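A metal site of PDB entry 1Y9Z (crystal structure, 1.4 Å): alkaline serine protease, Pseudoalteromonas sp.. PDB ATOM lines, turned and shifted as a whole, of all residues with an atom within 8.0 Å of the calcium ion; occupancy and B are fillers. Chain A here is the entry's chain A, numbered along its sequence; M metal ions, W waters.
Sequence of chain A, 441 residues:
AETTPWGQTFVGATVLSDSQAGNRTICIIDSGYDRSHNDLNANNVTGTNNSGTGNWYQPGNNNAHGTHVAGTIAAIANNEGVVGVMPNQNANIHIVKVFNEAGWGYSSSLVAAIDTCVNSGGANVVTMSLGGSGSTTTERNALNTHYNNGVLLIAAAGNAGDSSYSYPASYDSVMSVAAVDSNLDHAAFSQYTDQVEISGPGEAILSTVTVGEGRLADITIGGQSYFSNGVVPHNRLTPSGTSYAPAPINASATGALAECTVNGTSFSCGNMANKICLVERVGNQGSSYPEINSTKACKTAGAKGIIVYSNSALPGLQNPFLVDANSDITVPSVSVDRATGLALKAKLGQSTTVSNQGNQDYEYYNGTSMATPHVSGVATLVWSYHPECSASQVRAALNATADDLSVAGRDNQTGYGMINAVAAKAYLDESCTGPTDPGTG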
ATOM      1  N   ASP A 403       7.369 -19.527 -20.457  1.00  0.00           N
ATOM      2  CA  ASP A 403       8.590 -19.639 -19.658  1.00  0.00           C
ATOM      3  C   ASP A 403       8.850 -18.313 -18.936  1.00  0.00           C
ATOM      4  O   ASP A 403       9.150 -17.309 -19.569  1.00  0.00           O
ATOM      5  CB  ASP A 403       9.783 -20.002 -20.544  1.00  0.00           C
ATOM      6  CG  ASP A 403       9.588 -21.316 -21.277  1.00  0.00           C
ATOM      7  OD1 ASP A 403       9.130 -22.287 -20.649  1.00  0.00           O
ATOM      8  OD2 ASP A 403       9.904 -21.373 -22.483  1.00  0.00           O
ATOM      9  N   ASP A 404       8.741 -18.341 -17.613  1.00  0.00           N
ATOM     10  CA  ASP A 404       8.946 -17.163 -16.788  1.00  0.00           C
ATOM     11  C   ASP A 404      10.286 -16.482 -17.086  1.00  0.00           C
ATOM     12  O   ASP A 404      11.332 -17.130 -17.097  1.00  0.00           O
ATOM     13  CB  ASP A 404       8.882 -17.560 -15.311  1.00  0.00           C
ATOM     14  CG  ASP A 404       8.740 -16.371 -14.383  1.00  0.00           C
ATOM     15  OD1 ASP A 404       8.663 -15.223 -14.864  1.00  0.00           O
ATOM     16  OD2 ASP A 404       8.687 -16.588 -13.149  1.00  0.00           O
ATOM     17  N   LEU A 405      10.239 -15.174 -17.342  1.00  0.00           N
ATOM     18  CA  LEU A 405      11.431 -14.394 -17.642  1.00  0.00           C
ATOM     19  C   LEU A 405      11.605 -13.297 -16.594  1.00  0.00           C
ATOM     20  O   LEU A 405      10.696 -13.034 -15.813  1.00  0.00           O
ATOM     21  CB  LEU A 405      11.311 -13.732 -19.023  1.00  0.00           C
ATOM     22  CG  LEU A 405      11.063 -14.609 -20.260  1.00  0.00           C
ATOM     23  CD1 LEU A 405      11.036 -13.720 -21.502  1.00  0.00           C
ATOM     24  CD2 LEU A 405      12.155 -15.657 -20.376  1.00  0.00           C
ATOM     25  N   SER A 406      12.775 -12.673 -16.585  1.00  0.00           N
ATOM     26  CA  SER A 406      13.054 -11.590 -15.645  1.00  0.00           C
ATOM     27  C   SER A 406      12.765 -12.012 -14.206  1.00  0.00           C
ATOM     28  O   SER A 406      13.015 -13.160 -13.828  1.00  0.00           O
ATOM     29  CB  SER A 406      12.209 -10.363 -16.009  1.00  0.00           C
ATOM     30  OG  SER A 406      12.558  -9.231 -15.234  1.00  0.00           O
ATOM     31  N   VAL A 407      12.240 -11.096 -13.408  1.00  0.00           N
ATOM     32  CA  VAL A 407      11.914 -11.386 -12.018  1.00  0.00           C
ATOM     33  C   VAL A 407      10.869 -12.504 -11.961  1.00  0.00           C
ATOM     34  O   VAL A 407      10.027 -12.629 -12.853  1.00  0.00           O
ATOM     35  CB  VAL A 407      11.367 -10.132 -11.288  1.00  0.00           C
ATOM     36  CG1 VAL A 407      10.080  -9.667 -11.949  1.00  0.00           C
ATOM     37  CG2 VAL A 407      11.137 -10.445  -9.818  1.00  0.00           C
ATOM     38  N   ALA A 408      10.948 -13.321 -10.916  1.00  0.00           N
ATOM     39  CA  ALA A 408      10.012 -14.427 -10.744  1.00  0.00           C
ATOM     40  C   ALA A 408       8.566 -13.954 -10.776  1.00  0.00           C
ATOM     41  O   ALA A 408       8.222 -12.926 -10.180  1.00  0.00           O
ATOM     42  CB  ALA A 408      10.293 -15.143  -9.428  1.00  0.00           C
ATOM     43  N   GLY A 409       7.717 -14.709 -11.463  1.00  0.00           N
ATOM     44  CA  GLY A 409       6.311 -14.363 -11.561  1.00  0.00           C
ATOM     45  C   GLY A 409       6.008 -13.371 -12.666  1.00  0.00           C
ATOM     46  O   GLY A 409       6.906 -12.897 -13.352  1.00  0.00           O
ATOM     47  N   ARG A 410       4.730 -13.062 -12.822  1.00  0.00           N
ATOM     48  CA  ARG A 410       4.320 -12.117 -13.855  1.00  0.00           C
ATOM     49  C   ARG A 410       4.901 -10.735 -13.574  1.00  0.00           C
ATOM     50  O   ARG A 410       4.902 -10.282 -12.428  1.00  0.00           O
ATOM     51  CB  ARG A 410       2.800 -12.028 -13.923  1.00  0.00           C
ATOM     52  CG  ARG A 410       2.282 -11.111 -15.023  1.00  0.00           C
ATOM     53  CD  ARG A 410       0.769 -11.050 -15.043  1.00  0.00           C
ATOM     54  NE  ARG A 410       0.296 -10.275 -16.185  1.00  0.00           N
ATOM     55  CZ  ARG A 410      -0.963 -10.235 -16.605  1.00  0.00           C
ATOM     56  NH1 ARG A 410      -1.289  -9.499 -17.661  1.00  0.00           N
ATOM     57  NH2 ARG A 410      -1.907 -10.942 -15.985  1.00  0.00           N
ATOM     58  N   ASP A 411       5.419 -10.082 -14.610  1.00  0.00           N
ATOM     59  CA  ASP A 411       5.943  -8.728 -14.461  1.00  0.00           C
ATOM     60  C   ASP A 411       5.485  -7.876 -15.643  1.00  0.00           C
ATOM     61  O   ASP A 411       5.039  -8.420 -16.666  1.00  0.00           O
ATOM     62  CB  ASP A 411       7.474  -8.722 -14.338  1.00  0.00           C
ATOM     63  CG  ASP A 411       8.165  -9.483 -15.451  1.00  0.00           C
ATOM     64  OD1 ASP A 411       8.597 -10.628 -15.207  1.00  0.00           O
ATOM     65  OD2 ASP A 411       8.271  -8.924 -16.563  1.00  0.00           O
ATOM     66  N   ASN A 412       5.562  -6.565 -15.500  1.00  0.00           N
ATOM     67  CA  ASN A 412       5.118  -5.642 -16.541  1.00  0.00           C
ATOM     68  C   ASN A 412       5.963  -5.642 -17.804  1.00  0.00           C
ATOM     69  O   ASN A 412       5.490  -5.230 -18.864  1.00  0.00           O
ATOM     70  CB  ASN A 412       5.034  -4.218 -15.998  1.00  0.00           C
ATOM     71  CG  ASN A 412       3.943  -4.031 -14.951  1.00  0.00           C
ATOM     72  OD1 ASN A 412       3.666  -2.916 -14.521  1.00  0.00           O
ATOM     73  ND2 ASN A 412       3.322  -5.134 -14.534  1.00  0.00           N
ATOM     74  N   GLN A 413       7.205  -6.080 -17.694  1.00  0.00           N
ATOM     75  CA  GLN A 413       8.092  -6.112 -18.858  1.00  0.00           C
ATOM     76  C   GLN A 413       7.861  -7.298 -19.783  1.00  0.00           C
ATOM     77  O   GLN A 413       7.793  -7.140 -21.001  1.00  0.00           O
ATOM     78  CB  GLN A 413       9.565  -6.116 -18.415  1.00  0.00           C
ATOM     79  CG  GLN A 413      10.085  -4.766 -17.944  1.00  0.00           C
ATOM     80  CD  GLN A 413       9.543  -4.355 -16.590  1.00  0.00           C
ATOM     81  OE1 GLN A 413       9.418  -3.164 -16.305  1.00  0.00           O
ATOM     82  NE2 GLN A 413       9.254  -5.330 -15.740  1.00  0.00           N
ATOM     83  N   THR A 414       7.724  -8.485 -19.193  1.00  0.00           N
ATOM     84  CA  THR A 414       7.565  -9.706 -19.984  1.00  0.00           C
ATOM     85  C   THR A 414       6.283 -10.522 -19.767  1.00  0.00           C
ATOM     86  O   THR A 414       6.116 -11.589 -20.366  1.00  0.00           O
ATOM     87  CB  THR A 414       8.774 -10.638 -19.733  1.00  0.00           C
ATOM     88  OG1 THR A 414       8.808 -11.022 -18.347  1.00  0.00           O
ATOM     89  CG2 THR A 414      10.071  -9.920 -20.078  1.00  0.00           C
ATOM     90  N   GLY A 415       5.384 -10.026 -18.922  1.00  0.00           N
ATOM     91  CA  GLY A 415       4.162 -10.756 -18.655  1.00  0.00           C
ATOM     92  C   GLY A 415       4.479 -12.084 -17.987  1.00  0.00           C
ATOM     93  O   GLY A 415       5.295 -12.140 -17.074  1.00  0.00           O
ATOM     94  N   TYR A 416       3.844 -13.161 -18.452  1.00  0.00           N
ATOM     95  CA  TYR A 416       4.099 -14.481 -17.894  1.00  0.00           C
ATOM     96  C   TYR A 416       5.393 -15.087 -18.434  1.00  0.00           C
ATOM     97  O   TYR A 416       5.854 -16.119 -17.944  1.00  0.00           O
ATOM     98  CB  TYR A 416       2.916 -15.403 -18.164  1.00  0.00           C
ATOM     99  CG  TYR A 416       1.707 -15.069 -17.326  1.00  0.00           C
ATOM    100  CD1 TYR A 416       1.731 -15.204 -15.938  1.00  0.00           C
ATOM    101  CD2 TYR A 416       0.541 -14.578 -17.923  1.00  0.00           C
ATOM    102  CE1 TYR A 416       0.628 -14.854 -15.157  1.00  0.00           C
ATOM    103  CE2 TYR A 416      -0.564 -14.236 -17.147  1.00  0.00           C
ATOM    104  CZ  TYR A 416      -0.513 -14.375 -15.766  1.00  0.00           C
ATOM    105  OH  TYR A 416      -1.596 -14.008 -15.003  1.00  0.00           O
ATOM    106  N   GLY A 417       5.965 -14.450 -19.447  1.00  0.00           N
ATOM    107  CA  GLY A 417       7.216 -14.951 -20.008  1.00  0.00           C
ATOM    108  C   GLY A 417       7.170 -15.268 -21.481  1.00  0.00           C
ATOM    109  O   GLY A 417       6.279 -14.834 -22.213  1.00  0.00           O
ATOM    110  N   MET A 418       8.146 -16.049 -21.935  1.00  0.00           N
ATOM    111  CA  MET A 418       8.256 -16.425 -23.335  1.00  0.00           C
ATOM    112  C   MET A 418       7.253 -17.515 -23.708  1.00  0.00           C
ATOM    113  O   MET A 418       7.165 -18.537 -23.035  1.00  0.00           O
ATOM    114  CB  MET A 418       9.675 -16.924 -23.622  1.00  0.00           C
ATOM    115  CG  MET A 418       9.945 -17.169 -25.100  1.00  0.00           C
ATOM    116  SD  MET A 418       9.931 -15.630 -26.038  1.00  0.00           S
ATOM    117  CE  MET A 418      11.431 -15.807 -27.001  1.00  0.00           C
HETATM  118 CA    CA M   1       8.733 -12.895 -14.709  1.00  0.00          CA
HETATM  119  O   HOH W   1       7.872 -13.144 -16.946  1.00  0.00           O
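The backbone NH of Thr 414 is in hydrogen-bond range of the side-chain carboxylate of Asp 411 (2.7 Å).
The side-chain carboxylate (OD2) of Asp 411 sits close to the backbone NH (N) of Gln 413 (3.2 Å).
Five residues have an atom within 4 Å of the calcium ion: Asp 404, Leu 405, Val 407, Gly 409 and Asp 411.
The calcium ion is bound by the backbone carbonyl oxygen (O) of Leu 405, the backbone carbonyl oxygen (O) of Gly 409, the backbone carbonyl oxygen (O) of Val 407, the side-chain carboxylate (OD1) of Asp 411, the side-chain carboxylate (OD1) of Asp 404 and water W1.
Water W1 lies within hydrogen-bond range of OG1 of Thr 414 (2.7 Å), O of Gly 415 (2.8 Å), N of Leu 405 (3.1 Å) and N of Gly 417 (3.4 Å).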
